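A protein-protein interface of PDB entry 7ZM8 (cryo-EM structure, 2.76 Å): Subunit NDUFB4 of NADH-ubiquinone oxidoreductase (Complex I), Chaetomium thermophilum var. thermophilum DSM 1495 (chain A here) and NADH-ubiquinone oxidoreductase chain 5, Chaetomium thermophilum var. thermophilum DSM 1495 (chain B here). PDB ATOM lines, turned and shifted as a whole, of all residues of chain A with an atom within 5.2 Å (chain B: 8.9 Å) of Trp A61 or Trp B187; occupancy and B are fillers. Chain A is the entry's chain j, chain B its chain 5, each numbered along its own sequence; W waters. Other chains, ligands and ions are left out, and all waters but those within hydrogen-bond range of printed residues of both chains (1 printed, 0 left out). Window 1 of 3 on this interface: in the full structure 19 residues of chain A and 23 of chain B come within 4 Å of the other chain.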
ATOM      1  N   THR A  57      21.959   6.544  -4.544  1.00  0.00           N
ATOM      2  CA  THR A  57      21.559   7.136  -3.252  1.00  0.00           C
ATOM      3  C   THR A  57      21.082   8.568  -3.450  1.00  0.00           C
ATOM      4  O   THR A  57      20.921   9.260  -2.441  1.00  0.00           O
ATOM      5  CB  THR A  57      22.737   7.045  -2.278  1.00  0.00           C
ATOM      6  OG1 THR A  57      23.774   7.882  -2.783  1.00  0.00           O
ATOM      7  CG2 THR A  57      23.252   5.634  -2.112  1.00  0.00           C
ATOM      8  N   GLY A  59      18.811  11.619  -3.662  1.00  0.00           N
ATOM      9  CA  GLY A  59      17.445  11.889  -3.173  1.00  0.00           C
ATOM     10  C   GLY A  59      16.932  10.799  -2.251  1.00  0.00           C
ATOM     11  O   GLY A  59      15.727  10.779  -1.985  1.00  0.00           O
ATOM     12  N   LEU A  60      17.794   9.868  -1.853  1.00  0.00           N
ATOM     13  CA  LEU A  60      17.387   8.756  -0.956  1.00  0.00           C
ATOM     14  C   LEU A  60      17.048   9.261   0.448  1.00  0.00           C
ATOM     15  O   LEU A  60      16.107   8.729   1.042  1.00  0.00           O
ATOM     16  CB  LEU A  60      18.488   7.694  -0.917  1.00  0.00           C
ATOM     17  CG  LEU A  60      18.087   6.340  -0.339  1.00  0.00           C
ATOM     18  CD1 LEU A  60      16.753   5.879  -0.905  1.00  0.00           C
ATOM     19  CD2 LEU A  60      19.163   5.303  -0.609  1.00  0.00           C
ATOM     20  N   TRP A  61      17.795  10.231   0.970  1.00  0.00           N
ATOM     21  CA  TRP A  61      17.576  10.638   2.381  1.00  0.00           C
ATOM     22  C   TRP A  61      17.398  12.145   2.551  1.00  0.00           C
ATOM     23  O   TRP A  61      17.958  12.894   1.732  1.00  0.00           O
ATOM     24  CB  TRP A  61      18.750  10.170   3.248  1.00  0.00           C
ATOM     25  CG  TRP A  61      19.012   8.698   3.233  1.00  0.00           C
ATOM     26  CD1 TRP A  61      18.214   7.710   3.732  1.00  0.00           C
ATOM     27  CD2 TRP A  61      20.184   8.047   2.719  1.00  0.00           C
ATOM     28  NE1 TRP A  61      18.803   6.488   3.549  1.00  0.00           N
ATOM     29  CE2 TRP A  61      20.013   6.665   2.931  1.00  0.00           C
ATOM     30  CE3 TRP A  61      21.351   8.496   2.093  1.00  0.00           C
ATOM     31  CZ2 TRP A  61      20.970   5.731   2.542  1.00  0.00           C
ATOM     32  CZ3 TRP A  61      22.297   7.573   1.710  1.00  0.00           C
ATOM     33  CH2 TRP A  61      22.105   6.210   1.930  1.00  0.00           C
ATOM     34  N   ASP A  62      16.640  12.559   3.569  1.00  0.00           N
ATOM     35  CA  ASP A  62      16.499  13.988   3.927  1.00  0.00           C
ATOM     36  C   ASP A  62      16.395  14.031   5.441  1.00  0.00           C
ATOM     37  O   ASP A  62      15.659  13.223   6.000  1.00  0.00           O
ATOM     38  CB  ASP A  62      15.304  14.681   3.288  1.00  0.00           C
ATOM     39  CG  ASP A  62      15.123  16.120   3.728  1.00  0.00           C
ATOM     40  OD1 ASP A  62      16.094  16.888   3.619  1.00  0.00           O
ATOM     41  OD2 ASP A  62      14.013  16.454   4.186  1.00  0.00           O
ATOM     42  N   LEU A  63      17.086  14.959   6.100  1.00  0.00           N
ATOM     43  CA  LEU A  63      17.097  14.993   7.584  1.00  0.00           C
ATOM     44  C   LEU A  63      16.291  16.178   8.116  1.00  0.00           C
ATOM     45  O   LEU A  63      15.994  16.165   9.313  1.00  0.00           O
ATOM     46  CB  LEU A  63      18.547  15.139   8.057  1.00  0.00           C
ATOM     47  CG  LEU A  63      19.497  13.964   7.849  1.00  0.00           C
ATOM     48  CD1 LEU A  63      20.762  14.174   8.664  1.00  0.00           C
ATOM     49  CD2 LEU A  63      18.845  12.663   8.258  1.00  0.00           C
ATOM     50  N   ARG A  64      15.916  17.139   7.270  1.00  0.00           N
ATOM     51  CA  ARG A  64      15.311  18.356   7.792  1.00  0.00           C
ATOM     52  C   ARG A  64      13.960  18.078   8.432  1.00  0.00           C
ATOM     53  O   ARG A  64      13.090  17.443   7.829  1.00  0.00           O
ATOM     54  CB  ARG A  64      15.161  19.394   6.684  1.00  0.00           C
ATOM     55  CG  ARG A  64      14.724  20.769   7.176  1.00  0.00           C
ATOM     56  CD  ARG A  64      15.708  21.351   8.165  1.00  0.00           C
ATOM     57  NE  ARG A  64      16.880  21.917   7.509  1.00  0.00           N
ATOM     58  CZ  ARG A  64      16.977  23.173   7.089  1.00  0.00           C
ATOM     59  NH1 ARG A  64      18.084  23.593   6.506  1.00  0.00           N
ATOM     60  NH2 ARG A  64      15.969  24.010   7.245  1.00  0.00           N
ATOM     61  N   ALA A  65      13.804  18.544   9.671  1.00  0.00           N
ATOM     62  CA  ALA A  65      12.550  18.529  10.411  1.00  0.00           C
ATOM     63  C   ALA A  65      12.035  17.121  10.689  1.00  0.00           C
ATOM     64  O   ALA A  65      10.978  16.960  11.303  1.00  0.00           O
ATOM     65  CB  ALA A  65      11.494  19.348   9.668  1.00  0.00           C
ATOM     66  N   ILE A  72      13.793   8.699   7.723  1.00  0.00           N
ATOM     67  CA  ILE A  72      14.805   9.531   7.003  1.00  0.00           C
ATOM     68  C   ILE A  72      14.640   9.310   5.499  1.00  0.00           C
ATOM     69  O   ILE A  72      14.787  10.282   4.746  1.00  0.00           O
ATOM     70  CB  ILE A  72      16.240   9.208   7.486  1.00  0.00           C
ATOM     71  CG1 ILE A  72      16.359   9.260   9.010  1.00  0.00           C
ATOM     72  CG2 ILE A  72      17.265  10.095   6.809  1.00  0.00           C
ATOM     73  CD1 ILE A  72      17.719   8.870   9.527  1.00  0.00           C
ATOM     74  N   SER A  73      14.335   8.086   5.085  1.00  0.00           N
ATOM     75  CA  SER A  73      14.248   7.743   3.641  1.00  0.00           C
ATOM     76  C   SER A  73      13.153   8.505   2.890  1.00  0.00           C
ATOM     77  O   SER A  73      11.983   8.369   3.273  1.00  0.00           O
ATOM     78  CB  SER A  73      14.083   6.271   3.484  1.00  0.00           C
ATOM     79  OG  SER A  73      15.300   5.596   3.752  1.00  0.00           O
ATOM     80  N   GLU A  74      13.523   9.292   1.878  1.00  0.00           N
ATOM     81  CA  GLU A  74      12.544   9.961   1.033  1.00  0.00           C
ATOM     82  C   GLU A  74      11.824   8.981   0.124  1.00  0.00           C
ATOM     83  O   GLU A  74      10.620   9.118  -0.108  1.00  0.00           O
ATOM     84  CB  GLU A  74      13.219  11.018   0.160  1.00  0.00           C
ATOM     85  CG  GLU A  74      13.960  12.120   0.878  1.00  0.00           C
ATOM     86  CD  GLU A  74      14.558  13.110  -0.105  1.00  0.00           C
ATOM     87  OE1 GLU A  74      14.213  13.037  -1.305  1.00  0.00           O
ATOM     88  OE2 GLU A  74      15.373  13.959   0.305  1.00  0.00           O
ATOM     89  N   TRP B  69      18.287  30.234   7.675  1.00  0.00           N
ATOM     90  CA  TRP B  69      18.199  29.271   8.768  1.00  0.00           C
ATOM     91  C   TRP B  69      19.508  29.134   9.533  1.00  0.00           C
ATOM     92  O   TRP B  69      19.547  28.488  10.582  1.00  0.00           O
ATOM     93  CB  TRP B  69      17.767  27.894   8.250  1.00  0.00           C
ATOM     94  CG  TRP B  69      16.313  27.766   7.977  1.00  0.00           C
ATOM     95  CD1 TRP B  69      15.729  27.466   6.787  1.00  0.00           C
ATOM     96  CD2 TRP B  69      15.253  27.928   8.914  1.00  0.00           C
ATOM     97  NE1 TRP B  69      14.370  27.439   6.920  1.00  0.00           N
ATOM     98  CE2 TRP B  69      14.050  27.717   8.222  1.00  0.00           C
ATOM     99  CE3 TRP B  69      15.201  28.233  10.276  1.00  0.00           C
ATOM    100  CZ2 TRP B  69      12.813  27.804   8.841  1.00  0.00           C
ATOM    101  CZ3 TRP B  69      13.979  28.315  10.882  1.00  0.00           C
ATOM    102  CH2 TRP B  69      12.801  28.101  10.170  1.00  0.00           C
ATOM    103  N   PHE B  70      20.577  29.750   9.046  1.00  0.00           N
ATOM    104  CA  PHE B  70      21.877  29.713   9.701  1.00  0.00           C
ATOM    105  C   PHE B  70      22.159  31.094  10.272  1.00  0.00           C
ATOM    106  O   PHE B  70      22.368  32.048   9.519  1.00  0.00           O
ATOM    107  CB  PHE B  70      23.000  29.304   8.743  1.00  0.00           C
ATOM    108  CG  PHE B  70      22.909  27.892   8.224  1.00  0.00           C
ATOM    109  CD1 PHE B  70      21.788  27.108   8.442  1.00  0.00           C
ATOM    110  CD2 PHE B  70      23.966  27.347   7.516  1.00  0.00           C
ATOM    111  CE1 PHE B  70      21.714  25.820   7.956  1.00  0.00           C
ATOM    112  CE2 PHE B  70      23.897  26.054   7.032  1.00  0.00           C
ATOM    113  CZ  PHE B  70      22.767  25.292   7.255  1.00  0.00           C
ATOM    114  N   THR B 179      32.893  18.027  11.680  1.00  0.00           N
ATOM    115  CA  THR B 179      32.314  18.841  10.621  1.00  0.00           C
ATOM    116  C   THR B 179      31.137  18.122   9.974  1.00  0.00           C
ATOM    117  O   THR B 179      30.115  18.741   9.661  1.00  0.00           O
ATOM    118  CB  THR B 179      33.389  19.197   9.595  1.00  0.00           C
ATOM    119  OG1 THR B 179      34.431  19.935  10.239  1.00  0.00           O
ATOM    120  CG2 THR B 179      32.821  20.054   8.491  1.00  0.00           C
ATOM    121  N   VAL B 180      31.258  16.809   9.781  1.00  0.00           N
ATOM    122  CA  VAL B 180      30.132  16.008   9.315  1.00  0.00           C
ATOM    123  C   VAL B 180      29.023  15.988  10.357  1.00  0.00           C
ATOM    124  O   VAL B 180      27.837  16.061  10.023  1.00  0.00           O
ATOM    125  CB  VAL B 180      30.602  14.586   8.962  1.00  0.00           C
ATOM    126  CG1 VAL B 180      29.419  13.668   8.753  1.00  0.00           C
ATOM    127  CG2 VAL B 180      31.478  14.613   7.733  1.00  0.00           C
ATOM    128  N   GLY B 181      29.387  15.872  11.634  1.00  0.00           N
ATOM    129  CA  GLY B 181      28.386  15.868  12.684  1.00  0.00           C
ATOM    130  C   GLY B 181      27.655  17.185  12.833  1.00  0.00           C
ATOM    131  O   GLY B 181      26.459  17.199  13.129  1.00  0.00           O
ATOM    132  N   MET B 182      28.359  18.306  12.650  1.00  0.00           N
ATOM    133  CA  MET B 182      27.692  19.605  12.676  1.00  0.00           C
ATOM    134  C   MET B 182      26.856  19.837  11.429  1.00  0.00           C
ATOM    135  O   MET B 182      25.850  20.549  11.492  1.00  0.00           O
ATOM    136  CB  MET B 182      28.701  20.741  12.855  1.00  0.00           C
ATOM    137  CG  MET B 182      29.401  20.757  14.202  1.00  0.00           C
ATOM    138  SD  MET B 182      30.531  22.149  14.422  1.00  0.00           S
ATOM    139  CE  MET B 182      31.919  21.687  13.391  1.00  0.00           C
ATOM    140  N   PHE B 183      27.255  19.264  10.291  1.00  0.00           N
ATOM    141  CA  PHE B 183      26.405  19.324   9.105  1.00  0.00           C
ATOM    142  C   PHE B 183      25.086  18.616   9.351  1.00  0.00           C
ATOM    143  O   PHE B 183      24.030  19.090   8.921  1.00  0.00           O
ATOM    144  CB  PHE B 183      27.111  18.706   7.898  1.00  0.00           C
ATOM    145  CG  PHE B 183      28.237  19.528   7.364  1.00  0.00           C
ATOM    146  CD1 PHE B 183      28.344  20.870   7.670  1.00  0.00           C
ATOM    147  CD2 PHE B 183      29.191  18.958   6.545  1.00  0.00           C
ATOM    148  CE1 PHE B 183      29.384  21.620   7.182  1.00  0.00           C
ATOM    149  CE2 PHE B 183      30.234  19.707   6.058  1.00  0.00           C
ATOM    150  CZ  PHE B 183      30.326  21.044   6.375  1.00  0.00           C
ATOM    151  N   ALA B 184      25.163  17.476  10.048  1.00  0.00           N
ATOM    152  CA  ALA B 184      23.951  16.694  10.370  1.00  0.00           C
ATOM    153  C   ALA B 184      23.010  17.510  11.252  1.00  0.00           C
ATOM    154  O   ALA B 184      21.805  17.398  11.063  1.00  0.00           O
ATOM    155  CB  ALA B 184      24.334  15.393  11.015  1.00  0.00           C
ATOM    156  N   ILE B 185      23.567  18.254  12.215  1.00  0.00           N
ATOM    157  CA  ILE B 185      22.759  19.069  13.117  1.00  0.00           C
ATOM    158  C   ILE B 185      22.080  20.198  12.352  1.00  0.00           C
ATOM    159  O   ILE B 185      20.877  20.434  12.506  1.00  0.00           O
ATOM    160  CB  ILE B 185      23.624  19.609  14.271  1.00  0.00           C
ATOM    161  CG1 ILE B 185      24.144  18.468  15.140  1.00  0.00           C
ATOM    162  CG2 ILE B 185      22.848  20.589  15.120  1.00  0.00           C
ATOM    163  CD1 ILE B 185      25.120  18.921  16.203  1.00  0.00           C
ATOM    164  N   LEU B 186      22.837  20.908  11.511  1.00  0.00           N
ATOM    165  CA  LEU B 186      22.248  21.956  10.682  1.00  0.00           C
ATOM    166  C   LEU B 186      21.209  21.383   9.731  1.00  0.00           C
ATOM    167  O   LEU B 186      20.143  21.976   9.532  1.00  0.00           O
ATOM    168  CB  LEU B 186      23.330  22.679   9.881  1.00  0.00           C
ATOM    169  CG  LEU B 186      24.319  23.605  10.581  1.00  0.00           C
ATOM    170  CD1 LEU B 186      25.521  23.827   9.688  1.00  0.00           C
ATOM    171  CD2 LEU B 186      23.681  24.931  10.961  1.00  0.00           C
ATOM    172  N   TRP B 187      21.465  20.208   9.155  1.00  0.00           N
ATOM    173  CA  TRP B 187      20.534  19.569   8.192  1.00  0.00           C
ATOM    174  C   TRP B 187      19.238  19.168   8.897  1.00  0.00           C
ATOM    175  O   TRP B 187      18.198  19.398   8.321  1.00  0.00           O
ATOM    176  CB  TRP B 187      21.210  18.403   7.473  1.00  0.00           C
ATOM    177  CG  TRP B 187      20.475  17.879   6.280  1.00  0.00           C
ATOM    178  CD1 TRP B 187      19.383  18.422   5.671  1.00  0.00           C
ATOM    179  CD2 TRP B 187      20.792  16.688   5.543  1.00  0.00           C
ATOM    180  NE1 TRP B 187      18.995  17.648   4.614  1.00  0.00           N
ATOM    181  CE2 TRP B 187      19.841  16.578   4.509  1.00  0.00           C
ATOM    182  CE3 TRP B 187      21.785  15.709   5.655  1.00  0.00           C
ATOM    183  CZ2 TRP B 187      19.856  15.530   3.593  1.00  0.00           C
ATOM    184  CZ3 TRP B 187      21.796  14.673   4.752  1.00  0.00           C
ATOM    185  CH2 TRP B 187      20.842  14.586   3.740  1.00  0.00           C
ATOM    186  N   SER B 188      19.316  18.583  10.081  1.00  0.00           N
ATOM    187  CA  SER B 188      18.116  18.205  10.868  1.00  0.00           C
ATOM    188  C   SER B 188      17.375  19.365  11.531  1.00  0.00           C
ATOM    189  O   SER B 188      16.149  19.438  11.360  1.00  0.00           O
ATOM    190  CB  SER B 188      18.459  17.192  11.908  1.00  0.00           C
ATOM    191  OG  SER B 188      19.158  17.778  12.987  1.00  0.00           O
ATOM    192  N   LEU B 189      18.079  20.260  12.229  1.00  0.00           N
ATOM    193  CA  LEU B 189      17.386  21.273  13.074  1.00  0.00           C
ATOM    194  C   LEU B 189      17.489  22.684  12.526  1.00  0.00           C
ATOM    195  O   LEU B 189      16.825  23.534  13.057  1.00  0.00           O
ATOM    196  CB  LEU B 189      17.979  21.188  14.480  1.00  0.00           C
ATOM    197  CG  LEU B 189      17.742  19.883  15.231  1.00  0.00           C
ATOM    198  CD1 LEU B 189      18.358  19.964  16.615  1.00  0.00           C
ATOM    199  CD2 LEU B 189      16.257  19.583  15.321  1.00  0.00           C
ATOM    200  N   GLY B 190      18.360  22.926  11.563  1.00  0.00           N
ATOM    201  CA  GLY B 190      18.434  24.242  10.908  1.00  0.00           C
ATOM    202  C   GLY B 190      19.410  25.186  11.567  1.00  0.00           C
ATOM    203  O   GLY B 190      19.964  25.998  10.857  1.00  0.00           O
ATOM    204  N   ASN B 191      19.755  24.963  12.825  1.00  0.00           N
ATOM    205  CA  ASN B 191      20.770  25.816  13.479  1.00  0.00           C
ATOM    206  C   ASN B 191      21.527  24.972  14.486  1.00  0.00           C
ATOM    207  O   ASN B 191      20.912  24.077  15.065  1.00  0.00           O
ATOM    208  CB  ASN B 191      20.170  27.009  14.225  1.00  0.00           C
ATOM    209  CG  ASN B 191      20.989  28.274  14.091  1.00  0.00           C
ATOM    210  OD1 ASN B 191      21.698  28.462  13.110  1.00  0.00           O
ATOM    211  ND2 ASN B 191      20.880  29.154  15.068  1.00  0.00           N
ATOM    212  N   LEU B 192      22.817  25.240  14.647  1.00  0.00           N
ATOM    213  CA  LEU B 192      23.546  24.537  15.698  1.00  0.00           C
ATOM    214  C   LEU B 192      23.841  25.393  16.930  1.00  0.00           C
ATOM    215  O   LEU B 192      24.958  25.429  17.419  1.00  0.00           O
ATOM    216  CB  LEU B 192      24.809  23.936  15.085  1.00  0.00           C
ATOM    217  CG  LEU B 192      25.790  24.817  14.301  1.00  0.00           C
ATOM    218  CD1 LEU B 192      26.741  25.587  15.142  1.00  0.00           C
ATOM    219  CD2 LEU B 192      26.566  23.944  13.352  1.00  0.00           C
ATOM    220  N   ILE B 204      13.706  14.561  17.878  1.00  0.00           N
ATOM    221  CA  ILE B 204      14.375  14.258  16.619  1.00  0.00           C
ATOM    222  C   ILE B 204      14.347  12.758  16.342  1.00  0.00           C
ATOM    223  O   ILE B 204      14.308  11.927  17.254  1.00  0.00           O
ATOM    224  CB  ILE B 204      15.822  14.775  16.658  1.00  0.00           C
ATOM    225  CG1 ILE B 204      15.861  16.203  17.189  1.00  0.00           C
ATOM    226  CG2 ILE B 204      16.468  14.713  15.288  1.00  0.00           C
ATOM    227  CD1 ILE B 204      17.262  16.703  17.450  1.00  0.00           C
ATOM    228  N   VAL B 208      18.762   9.877  13.412  1.00  0.00           N
ATOM    229  CA  VAL B 208      19.516  11.112  13.230  1.00  0.00           C
ATOM    230  C   VAL B 208      20.401  11.373  14.441  1.00  0.00           C
ATOM    231  O   VAL B 208      21.529  11.857  14.310  1.00  0.00           O
ATOM    232  CB  VAL B 208      18.552  12.282  12.951  1.00  0.00           C
ATOM    233  CG1 VAL B 208      19.267  13.616  13.072  1.00  0.00           C
ATOM    234  CG2 VAL B 208      17.942  12.141  11.572  1.00  0.00           C
ATOM    235  N   ILE B 211      23.564   9.333  14.081  1.00  0.00           N
ATOM    236  CA  ILE B 211      24.575   9.929  13.168  1.00  0.00           C
ATOM    237  C   ILE B 211      25.344  11.036  13.879  1.00  0.00           C
ATOM    238  O   ILE B 211      26.575  11.049  13.783  1.00  0.00           O
ATOM    239  CB  ILE B 211      23.920  10.429  11.872  1.00  0.00           C
ATOM    240  CG1 ILE B 211      23.130   9.317  11.180  1.00  0.00           C
ATOM    241  CG2 ILE B 211      24.948  11.057  10.946  1.00  0.00           C
ATOM    242  CD1 ILE B 211      22.415   9.766   9.932  1.00  0.00           C
ATOM    243  N   ILE B 212      24.636  11.915  14.592  1.00  0.00           N
ATOM    244  CA  ILE B 212      25.324  12.998  15.285  1.00  0.00           C
ATOM    245  C   ILE B 212      26.193  12.450  16.407  1.00  0.00           C
ATOM    246  O   ILE B 212      27.348  12.858  16.572  1.00  0.00           O
ATOM    247  CB  ILE B 212      24.309  14.025  15.809  1.00  0.00           C
ATOM    248  CG1 ILE B 212      23.497  14.606  14.653  1.00  0.00           C
ATOM    249  CG2 ILE B 212      25.021  15.112  16.577  1.00  0.00           C
ATOM    250  CD1 ILE B 212      22.272  15.365  15.098  1.00  0.00           C
HETATM  251  O   HOH W   1      13.484  24.507   6.322  1.00  0.00           O
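OD1 of Asp A62 lies within hydrogen-bond range of NE1 of Trp B187, 3.2 Å away.
The guanidinium group of Arg A64 lies within hydrogen-bond range of the backbone carbonyl oxygen of Trp B187 (3.0 Å).
N of Ala A65 is in hydrogen-bond range of O of Ser B188 (3.0 Å).
Trp A61 touches one residue of chain B.
Printed residues of chain B within 4 Å of Asp A62: Trp B187 (3.2 Å).
Of the printed residues of chain B, Arg A64 touches Trp B69, Leu B186, Trp B187 and Ser B188.
Printed residues of chain A within 4 Å of Trp B69: Arg A64.
Printed residues of chain A within 4 Å of Leu B186: Arg A64 (3.8 Å).
Printed residues of chain A within 4 Å of Trp B187: Trp A61 (3.7 Å), Asp A62 (3.2 Å), Leu A63 (3.5 Å) and Arg A64 (3.0 Å).
Of the printed residues of chain A, Ser B188 touches Leu A63 (3.3 Å), Arg A64 (3.7 Å) and Ala A65 (3.0 Å).
Leu B189 touches none of the printed residues of chain A.
The nearest residue of chain B that does not touch Trp A61 is Ile B211 (7.6 Å).
Among the printed residues, pairs that only touch across the chains: Leu A63 with Ser B188, Leu A63 with Val B208, Arg A64 with Trp B69, Leu A63 with Trp B187, Trp A61 with Trp B187, Arg A64 with Ser B188, Arg A64 with Leu B186 and Ile A72 with Val B208.
The backbone NH of Asp A62 lies within hydrogen-bond range of the backbone carbonyl oxygen of Ile A72, at 3.2 Å.
O of Gly B190 sits close to O of Trp B69.
The side-chain amide oxygen (OD1) of Asn B191 sits close to the backbone carbonyl oxygen (O) of Trp B69.
The backbone carbonyl oxygen (O) of Ala B184 lies within hydrogen-bond range of the side-chain hydroxyl (OG) of Ser B188 (3.3 Å).
The backbone carbonyl oxygen (O) of Ile B185 lies within hydrogen-bond range of the side-chain hydroxyl (OG) of Ser B188, at 3.2 Å.
Water W1 bridges NH2 of Arg A64 (2.7 Å) and NE1 of Trp B69 (3.1 Å).
Of the 11 printed residues of chain A, 6 touch a printed residue of chain B.
Hydrophobic or aromatic side chains of chain A within 4 Å of the printed part of chain B: Leu A63 and Ile A72.
Among the printed residues, 11 pairs touch across the chains.
Among the printed residues, no Asp or Glu carboxylate lies within 4 Å of a Lys or Arg side-chain nitrogen of the other chain.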
